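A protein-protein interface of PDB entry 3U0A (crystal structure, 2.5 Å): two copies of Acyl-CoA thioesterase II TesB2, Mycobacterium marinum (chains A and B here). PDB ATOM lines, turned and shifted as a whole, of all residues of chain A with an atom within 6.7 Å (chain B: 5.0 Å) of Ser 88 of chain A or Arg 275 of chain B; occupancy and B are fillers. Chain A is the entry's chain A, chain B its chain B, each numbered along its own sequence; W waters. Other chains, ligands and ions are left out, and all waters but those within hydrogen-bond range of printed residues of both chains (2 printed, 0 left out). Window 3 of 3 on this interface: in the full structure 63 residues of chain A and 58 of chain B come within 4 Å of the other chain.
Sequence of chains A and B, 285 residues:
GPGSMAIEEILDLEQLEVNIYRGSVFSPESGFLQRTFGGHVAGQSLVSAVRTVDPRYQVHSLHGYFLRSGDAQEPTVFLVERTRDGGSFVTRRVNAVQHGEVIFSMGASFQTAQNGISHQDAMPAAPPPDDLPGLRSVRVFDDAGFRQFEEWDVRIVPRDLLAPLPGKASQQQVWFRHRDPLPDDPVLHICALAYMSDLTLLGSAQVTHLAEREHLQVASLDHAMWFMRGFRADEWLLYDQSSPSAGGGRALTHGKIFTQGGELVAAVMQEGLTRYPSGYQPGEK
The guanidinium group (NH1) of Arg 275 of chain B lies within hydrogen-bond range of the side-chain amide oxygen (OE1) of Gln 114 of chain A (2.9 Å). OG of Ser 88 of chain A lies within hydrogen-bond range of NH1 of Arg 275 of chain B (3.4 Å). O of Asn 115 of chain A lies within hydrogen-bond range of N of Tyr 276 of chain B.
The backbone carbonyl oxygen (O) of Arg 275 of chain B sits at hydrogen-bond distance from the backbone NH (N) of Gln 217 of chain B (2.8 Å). The side-chain hydroxyl (OG1) of Thr 112 of chain A lies within hydrogen-bond range of the side-chain amide nitrogen (NE2) of Gln 114 of chain A, at 3.4 Å. The backbone NH (N) of Thr 112 of chain A lies within hydrogen-bond range of the backbone carbonyl oxygen (O) of Ser 88 of chain A (3.0 Å). The side-chain hydroxyl (OG) of Ser 88 of chain A is in hydrogen-bond range of the side-chain amide nitrogen (NE2) of Gln 114 of chain A (2.9 Å). The backbone carbonyl oxygen of Gly 249 of chain B is in hydrogen-bond range of the backbone NH of Thr 274 of chain B, 2.8 Å away. NE2 of Gln 111 of chain A is in hydrogen-bond range of OE1 of Gln 114 of chain A (3.2 Å).
CE1 of Phe 89 of chain A touches CD1 of Leu 273 of chain B, at 3.7 Å. CE1 of Phe 89 of chain A touches NH1 of Arg 275 of chain B, 3.8 Å away. Gly 249 of chain B touches Asn 115 of chain A. CA of Arg 275 of chain B touches O of Asn 115 of chain A (3.3 Å). Gly 116 of chain A touches Gly 249 of chain B (N to N, 3.7 Å). Gly 116 of chain A touches Thr 274 of chain B. Gly 116 of chain A touches Tyr 276 of chain B. Ile 117 of chain A touches Leu 216 of chain B (CG2 to CD1, 3.9 Å). Thr 274 of chain B touches Ile 117 of chain A. Ile 117 of chain A touches Tyr 276 of chain B.
Gly 87 of chain A touches none of the printed residues of chain B. Printed residues of chain B within 4 Å of Ser 88 of chain A: Arg 275 (3.4 Å). Of the printed residues of chain A, Leu 273 of chain B touches Phe 89. Arg 275 of chain B touches four residues of chain A. Of the printed residues of chain A, Tyr 276 of chain B touches Asn 115, Gly 116 and Ile 117. Pro 277 of chain B touches none of the printed residues of chain A. The nearest residue of chain A that does not touch Arg 275 of chain B is Gly 116 of chain A (4.3 Å). The nearest printed residue of chain B that does not touch Ile 117 of chain A is Gly 249 of chain B (5.4 Å).
Of the 16 printed residues of chain A, 6 touch a printed residue of chain B. Printed residues of chain B that touch a printed residue of chain A: Leu 216, Gly 249, Leu 273, Thr 274, Arg 275 and Tyr 276. Hydrophobic or aromatic side chains of chain B that line the printed part of chain A: Leu 216, Leu 273 and Tyr 276. Along chain B the printed residues that touch a printed residue of chain A span positions 216 to 276. Among the printed residues, 13 pairs touch across the chains.
No position is printed for both chains. Of the 13 pairs that touch across the chains among the printed residues, none has its exchanged pair printed and touching as well.
Water W1 lies within hydrogen-bond range of the backbone carbonyl oxygen of Ile 117 of chain A (2.7 Å), the backbone NH of Gly 249 of chain B (3.0 Å) and the side-chain hydroxyl of Thr 274 of chain B (3.2 Å). Water W2 bridges N of Asn 115 of chain A (3.0 Å) and O of Tyr 276 of chain B (3.0 Å).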
ATOM      1  N   ARG A  56       2.318   3.268 -16.635  1.00  0.00           N
ATOM      2  CA  ARG A  56       3.642   2.930 -16.072  1.00  0.00           C
ATOM      3  C   ARG A  56       3.588   1.678 -15.152  1.00  0.00           C
ATOM      4  O   ARG A  56       4.598   0.998 -14.936  1.00  0.00           O
ATOM      5  CB  ARG A  56       4.240   4.142 -15.309  1.00  0.00           C
ATOM      6  N   TYR A  57       2.409   1.380 -14.621  1.00  0.00           N
ATOM      7  CA  TYR A  57       2.222   0.212 -13.784  1.00  0.00           C
ATOM      8  C   TYR A  57       1.469  -0.835 -14.560  1.00  0.00           C
ATOM      9  O   TYR A  57       0.389  -0.568 -15.084  1.00  0.00           O
ATOM     10  CB  TYR A  57       1.415   0.534 -12.539  1.00  0.00           C
ATOM     11  CG  TYR A  57       1.920   1.677 -11.696  1.00  0.00           C
ATOM     12  CD1 TYR A  57       1.776   2.981 -12.122  1.00  0.00           C
ATOM     13  CD2 TYR A  57       2.474   1.452 -10.440  1.00  0.00           C
ATOM     14  CE1 TYR A  57       2.183   4.033 -11.349  1.00  0.00           C
ATOM     15  CE2 TYR A  57       2.873   2.495  -9.644  1.00  0.00           C
ATOM     16  CZ  TYR A  57       2.734   3.792 -10.109  1.00  0.00           C
ATOM     17  OH  TYR A  57       3.141   4.867  -9.330  1.00  0.00           O
ATOM     18  N   ASP A  85      -2.786   3.814  -4.342  1.00  0.00           N
ATOM     19  CA  ASP A  85      -1.922   4.371  -5.365  1.00  0.00           C
ATOM     20  C   ASP A  85      -0.548   4.803  -4.753  1.00  0.00           C
ATOM     21  O   ASP A  85      -0.402   5.902  -4.260  1.00  0.00           O
ATOM     22  CB  ASP A  85      -2.618   5.568  -6.044  1.00  0.00           C
ATOM     23  CG  ASP A  85      -3.705   5.141  -7.004  1.00  0.00           C
ATOM     24  OD1 ASP A  85      -3.458   5.135  -8.217  1.00  0.00           O
ATOM     25  OD2 ASP A  85      -4.808   4.771  -6.550  1.00  0.00           O
ATOM     26  N   GLY A  86       0.434   3.922  -4.789  1.00  0.00           N
ATOM     27  CA  GLY A  86       1.745   4.227  -4.250  1.00  0.00           C
ATOM     28  C   GLY A  86       2.753   4.419  -5.353  1.00  0.00           C
ATOM     29  O   GLY A  86       2.391   4.572  -6.522  1.00  0.00           O
ATOM     30  N   GLY A  87       4.026   4.394  -4.981  1.00  0.00           N
ATOM     31  CA  GLY A  87       5.117   4.667  -5.911  1.00  0.00           C
ATOM     32  C   GLY A  87       5.467   3.525  -6.853  1.00  0.00           C
ATOM     33  O   GLY A  87       5.894   3.770  -7.971  1.00  0.00           O
ATOM     34  N   SER A  88       5.302   2.294  -6.376  1.00  0.00           N
ATOM     35  CA  SER A  88       5.657   1.083  -7.122  1.00  0.00           C
ATOM     36  C   SER A  88       4.450   0.226  -7.444  1.00  0.00           C
ATOM     37  O   SER A  88       4.442  -0.465  -8.458  1.00  0.00           O
ATOM     38  CB  SER A  88       6.637   0.212  -6.319  1.00  0.00           C
ATOM     39  OG  SER A  88       7.901   0.837  -6.239  1.00  0.00           O
ATOM     40  N   PHE A  89       3.452   0.257  -6.566  1.00  0.00           N
ATOM     41  CA  PHE A  89       2.298  -0.578  -6.708  1.00  0.00           C
ATOM     42  C   PHE A  89       0.991   0.250  -6.671  1.00  0.00           C
ATOM     43  O   PHE A  89       0.845   1.211  -5.889  1.00  0.00           O
ATOM     44  CB  PHE A  89       2.296  -1.632  -5.592  1.00  0.00           C
ATOM     45  CG  PHE A  89       3.352  -2.715  -5.756  1.00  0.00           C
ATOM     46  CD1 PHE A  89       4.640  -2.517  -5.290  1.00  0.00           C
ATOM     47  CD2 PHE A  89       3.047  -3.938  -6.365  1.00  0.00           C
ATOM     48  CE1 PHE A  89       5.600  -3.485  -5.433  1.00  0.00           C
ATOM     49  CE2 PHE A  89       4.023  -4.912  -6.512  1.00  0.00           C
ATOM     50  CZ  PHE A  89       5.300  -4.678  -6.037  1.00  0.00           C
ATOM     51  N   VAL A  90       0.046  -0.124  -7.527  1.00  0.00           N
ATOM     52  CA  VAL A  90      -1.290   0.415  -7.485  1.00  0.00           C
ATOM     53  C   VAL A  90      -2.231  -0.777  -7.332  1.00  0.00           C
ATOM     54  O   VAL A  90      -1.994  -1.857  -7.888  1.00  0.00           O
ATOM     55  CB  VAL A  90      -1.576   1.242  -8.756  1.00  0.00           C
ATOM     56  CG1 VAL A  90      -3.054   1.503  -8.931  1.00  0.00           C
ATOM     57  CG2 VAL A  90      -0.802   2.567  -8.736  1.00  0.00           C
ATOM     58  N   PHE A 110      -1.011  -3.748  -9.654  1.00  0.00           N
ATOM     59  CA  PHE A 110      -0.216  -3.190 -10.739  1.00  0.00           C
ATOM     60  C   PHE A 110       1.154  -2.651 -10.210  1.00  0.00           C
ATOM     61  O   PHE A 110       1.225  -2.000  -9.162  1.00  0.00           O
ATOM     62  CB  PHE A 110      -1.016  -2.067 -11.427  1.00  0.00           C
ATOM     63  CG  PHE A 110      -2.397  -2.487 -11.894  1.00  0.00           C
ATOM     64  CD1 PHE A 110      -3.394  -2.765 -10.988  1.00  0.00           C
ATOM     65  CD2 PHE A 110      -2.688  -2.587 -13.244  1.00  0.00           C
ATOM     66  CE1 PHE A 110      -4.647  -3.155 -11.400  1.00  0.00           C
ATOM     67  CE2 PHE A 110      -3.955  -2.984 -13.676  1.00  0.00           C
ATOM     68  CZ  PHE A 110      -4.937  -3.274 -12.746  1.00  0.00           C
ATOM     69  N   GLN A 111       2.233  -2.940 -10.935  1.00  0.00           N
ATOM     70  CA  GLN A 111       3.574  -2.575 -10.500  1.00  0.00           C
ATOM     71  C   GLN A 111       4.356  -1.957 -11.613  1.00  0.00           C
ATOM     72  O   GLN A 111       4.193  -2.308 -12.771  1.00  0.00           O
ATOM     73  CB  GLN A 111       4.321  -3.814 -10.002  1.00  0.00           C
ATOM     74  CG  GLN A 111       5.739  -3.568  -9.459  1.00  0.00           C
ATOM     75  CD  GLN A 111       6.562  -4.845  -9.321  1.00  0.00           C
ATOM     76  OE1 GLN A 111       6.296  -5.824  -9.983  1.00  0.00           O
ATOM     77  NE2 GLN A 111       7.558  -4.830  -8.450  1.00  0.00           N
ATOM     78  N   THR A 112       5.263  -1.069 -11.251  1.00  0.00           N
ATOM     79  CA  THR A 112       6.229  -0.548 -12.226  1.00  0.00           C
ATOM     80  C   THR A 112       7.317  -1.593 -12.591  1.00  0.00           C
ATOM     81  O   THR A 112       7.460  -2.654 -11.977  1.00  0.00           O
ATOM     82  CB  THR A 112       6.883   0.779 -11.765  1.00  0.00           C
ATOM     83  OG1 THR A 112       7.406   0.618 -10.451  1.00  0.00           O
ATOM     84  CG2 THR A 112       5.898   1.904 -11.762  1.00  0.00           C
ATOM     85  N   ALA A 113       8.068  -1.283 -13.640  1.00  0.00           N
ATOM     86  CA  ALA A 113       9.188  -2.130 -14.044  1.00  0.00           C
ATOM     87  C   ALA A 113      10.299  -1.994 -13.017  1.00  0.00           C
ATOM     88  O   ALA A 113      10.806  -0.917 -12.813  1.00  0.00           O
ATOM     89  CB  ALA A 113       9.688  -1.747 -15.440  1.00  0.00           C
ATOM     90  N   GLN A 114      10.625  -3.090 -12.347  1.00  0.00           N
ATOM     91  CA  GLN A 114      11.703  -3.104 -11.371  1.00  0.00           C
ATOM     92  C   GLN A 114      12.472  -4.430 -11.471  1.00  0.00           C
ATOM     93  O   GLN A 114      12.221  -5.217 -12.373  1.00  0.00           O
ATOM     94  CB  GLN A 114      11.125  -2.885  -9.969  1.00  0.00           C
ATOM     95  CG  GLN A 114      10.072  -1.781  -9.930  1.00  0.00           C
ATOM     96  CD  GLN A 114       9.668  -1.370  -8.521  1.00  0.00           C
ATOM     97  OE1 GLN A 114       9.180  -2.199  -7.717  1.00  0.00           O
ATOM     98  NE2 GLN A 114       9.846  -0.077  -8.213  1.00  0.00           N
ATOM     99  N   ASN A 115      13.382  -4.686 -10.529  1.00  0.00           N
ATOM    100  CA  ASN A 115      14.300  -5.830 -10.629  1.00  0.00           C
ATOM    101  C   ASN A 115      14.391  -6.653  -9.343  1.00  0.00           C
ATOM    102  O   ASN A 115      14.052  -6.181  -8.269  1.00  0.00           O
ATOM    103  CB  ASN A 115      15.704  -5.335 -11.059  1.00  0.00           C
ATOM    104  CG  ASN A 115      15.647  -4.403 -12.275  1.00  0.00           C
ATOM    105  OD1 ASN A 115      15.820  -3.166 -12.151  1.00  0.00           O
ATOM    106  ND2 ASN A 115      15.362  -4.988 -13.466  1.00  0.00           N
ATOM    107  N   GLY A 116      14.869  -7.881  -9.482  1.00  0.00           N
ATOM    108  CA  GLY A 116      14.911  -8.803  -8.375  1.00  0.00           C
ATOM    109  C   GLY A 116      15.493 -10.147  -8.723  1.00  0.00           C
ATOM    110  O   GLY A 116      15.914 -10.384  -9.854  1.00  0.00           O
ATOM    111  N   ILE A 117      15.572 -11.029  -7.747  1.00  0.00           N
ATOM    112  CA  ILE A 117      15.991 -12.388  -8.014  1.00  0.00           C
ATOM    113  C   ILE A 117      15.222 -12.972  -9.182  1.00  0.00           C
ATOM    114  O   ILE A 117      14.054 -12.604  -9.429  1.00  0.00           O
ATOM    115  CB  ILE A 117      15.764 -13.285  -6.815  1.00  0.00           C
ATOM    116  CG1 ILE A 117      14.304 -13.202  -6.345  1.00  0.00           C
ATOM    117  CG2 ILE A 117      16.698 -12.873  -5.701  1.00  0.00           C
ATOM    118  CD1 ILE A 117      13.971 -14.108  -5.184  1.00  0.00           C
ATOM    119  N   HIS B 215      20.479  -7.703   0.043  1.00  0.00           N
ATOM    120  CA  HIS B 215      20.202  -6.656  -0.912  1.00  0.00           C
ATOM    121  C   HIS B 215      18.776  -6.734  -1.362  1.00  0.00           C
ATOM    122  O   HIS B 215      18.384  -6.040  -2.293  1.00  0.00           O
ATOM    123  CB  HIS B 215      21.161  -6.784  -2.108  1.00  0.00           C
ATOM    124  CG  HIS B 215      22.612  -6.998  -1.701  1.00  0.00           C
ATOM    125  ND1 HIS B 215      23.062  -8.173  -1.191  1.00  0.00           N
ATOM    126  CD2 HIS B 215      23.701  -6.137  -1.712  1.00  0.00           C
ATOM    127  CE1 HIS B 215      24.370  -8.063  -0.895  1.00  0.00           C
ATOM    128  NE2 HIS B 215      24.763  -6.824  -1.223  1.00  0.00           N
ATOM    129  N   LEU B 216      17.980  -7.570  -0.704  1.00  0.00           N
ATOM    130  CA  LEU B 216      16.590  -7.759  -1.082  1.00  0.00           C
ATOM    131  C   LEU B 216      15.630  -6.986  -0.200  1.00  0.00           C
ATOM    132  O   LEU B 216      15.725  -7.042   1.000  1.00  0.00           O
ATOM    133  CB  LEU B 216      16.241  -9.224  -1.013  1.00  0.00           C
ATOM    134  CG  LEU B 216      16.653  -9.969  -2.249  1.00  0.00           C
ATOM    135  CD1 LEU B 216      16.255 -11.409  -2.075  1.00  0.00           C
ATOM    136  CD2 LEU B 216      16.002  -9.342  -3.472  1.00  0.00           C
ATOM    137  N   GLN B 217      14.726  -6.242  -0.829  1.00  0.00           N
ATOM    138  CA  GLN B 217      13.511  -5.765  -0.183  1.00  0.00           C
ATOM    139  C   GLN B 217      12.431  -6.856  -0.296  1.00  0.00           C
ATOM    140  O   GLN B 217      12.041  -7.236  -1.404  1.00  0.00           O
ATOM    141  CB  GLN B 217      13.040  -4.486  -0.853  1.00  0.00           C
ATOM    142  CG  GLN B 217      13.901  -3.290  -0.524  1.00  0.00           C
ATOM    143  CD  GLN B 217      13.528  -2.025  -1.317  1.00  0.00           C
ATOM    144  OE1 GLN B 217      12.641  -1.232  -0.898  1.00  0.00           O
ATOM    145  NE2 GLN B 217      14.210  -1.816  -2.453  1.00  0.00           N
ATOM    146  N   GLY B 249      11.156  -8.108  -9.736  1.00  0.00           N
ATOM    147  CA  GLY B 249      11.150  -7.749  -8.344  1.00  0.00           C
ATOM    148  C   GLY B 249      10.102  -8.413  -7.481  1.00  0.00           C
ATOM    149  O   GLY B 249       9.815  -7.919  -6.380  1.00  0.00           O
ATOM    150  N   LEU B 273       7.139  -9.283  -2.643  1.00  0.00           N
ATOM    151  CA  LEU B 273       8.236  -8.420  -3.096  1.00  0.00           C
ATOM    152  C   LEU B 273       9.603  -9.062  -2.862  1.00  0.00           C
ATOM    153  O   LEU B 273       9.884  -9.505  -1.769  1.00  0.00           O
ATOM    154  CB  LEU B 273       8.176  -7.101  -2.318  1.00  0.00           C
ATOM    155  CG  LEU B 273       9.070  -5.924  -2.721  1.00  0.00           C
ATOM    156  CD1 LEU B 273       8.486  -5.238  -3.959  1.00  0.00           C
ATOM    157  CD2 LEU B 273       9.224  -4.963  -1.535  1.00  0.00           C
ATOM    158  N   THR B 274      10.425  -9.150  -3.904  1.00  0.00           N
ATOM    159  CA  THR B 274      11.811  -9.618  -3.755  1.00  0.00           C
ATOM    160  C   THR B 274      12.745  -8.780  -4.606  1.00  0.00           C
ATOM    161  O   THR B 274      13.206  -9.222  -5.658  1.00  0.00           O
ATOM    162  CB  THR B 274      11.955 -11.101  -4.121  1.00  0.00           C
ATOM    163  OG1 THR B 274      11.726 -11.312  -5.527  1.00  0.00           O
ATOM    164  CG2 THR B 274      10.969 -11.891  -3.361  1.00  0.00           C
ATOM    165  N   ARG B 275      13.019  -7.570  -4.139  1.00  0.00           N
ATOM    166  CA  ARG B 275      13.451  -6.485  -5.012  1.00  0.00           C
ATOM    167  C   ARG B 275      14.845  -5.995  -4.694  1.00  0.00           C
ATOM    168  O   ARG B 275      15.191  -5.803  -3.527  1.00  0.00           O
ATOM    169  CB  ARG B 275      12.485  -5.317  -4.854  1.00  0.00           C
ATOM    170  CG  ARG B 275      12.636  -4.182  -5.856  1.00  0.00           C
ATOM    171  CD  ARG B 275      11.396  -3.286  -5.800  1.00  0.00           C
ATOM    172  NE  ARG B 275      11.250  -2.665  -4.486  1.00  0.00           N
ATOM    173  CZ  ARG B 275      10.158  -2.052  -4.044  1.00  0.00           C
ATOM    174  NH1 ARG B 275       9.070  -1.980  -4.795  1.00  0.00           N
ATOM    175  NH2 ARG B 275      10.146  -1.530  -2.825  1.00  0.00           N
ATOM    176  N   TYR B 276      15.640  -5.793  -5.744  1.00  0.00           N
ATOM    177  CA  TYR B 276      16.914  -5.080  -5.623  1.00  0.00           C
ATOM    178  C   TYR B 276      16.622  -3.593  -5.519  1.00  0.00           C
ATOM    179  O   TYR B 276      15.676  -3.126  -6.155  1.00  0.00           O
ATOM    180  CB  TYR B 276      17.845  -5.304  -6.829  1.00  0.00           C
ATOM    181  CG  TYR B 276      18.272  -6.727  -7.070  1.00  0.00           C
ATOM    182  CD1 TYR B 276      18.400  -7.640  -6.018  1.00  0.00           C
ATOM    183  CD2 TYR B 276      18.538  -7.172  -8.356  1.00  0.00           C
ATOM    184  CE1 TYR B 276      18.773  -8.959  -6.248  1.00  0.00           C
ATOM    185  CE2 TYR B 276      18.909  -8.485  -8.596  1.00  0.00           C
ATOM    186  CZ  TYR B 276      19.045  -9.375  -7.546  1.00  0.00           C
ATOM    187  OH  TYR B 276      19.435 -10.679  -7.828  1.00  0.00           O
ATOM    188  N   PRO B 277      17.384  -2.860  -4.671  1.00  0.00           N
ATOM    189  CA  PRO B 277      17.405  -1.407  -4.637  1.00  0.00           C
ATOM    190  C   PRO B 277      17.641  -0.803  -6.004  1.00  0.00           C
ATOM    191  O   PRO B 277      17.857  -1.547  -6.972  1.00  0.00           O
ATOM    192  CB  PRO B 277      18.563  -1.126  -3.691  1.00  0.00           C
ATOM    193  CG  PRO B 277      18.397  -2.186  -2.645  1.00  0.00           C
ATOM    194  CD  PRO B 277      17.854  -3.400  -3.378  1.00  0.00           C
HETATM  195  O   HOH W   1      12.344 -10.664  -8.649  1.00  0.00           O
HETATM  196  O   HOH W   2      14.300  -2.479  -8.789  1.00  0.00           O
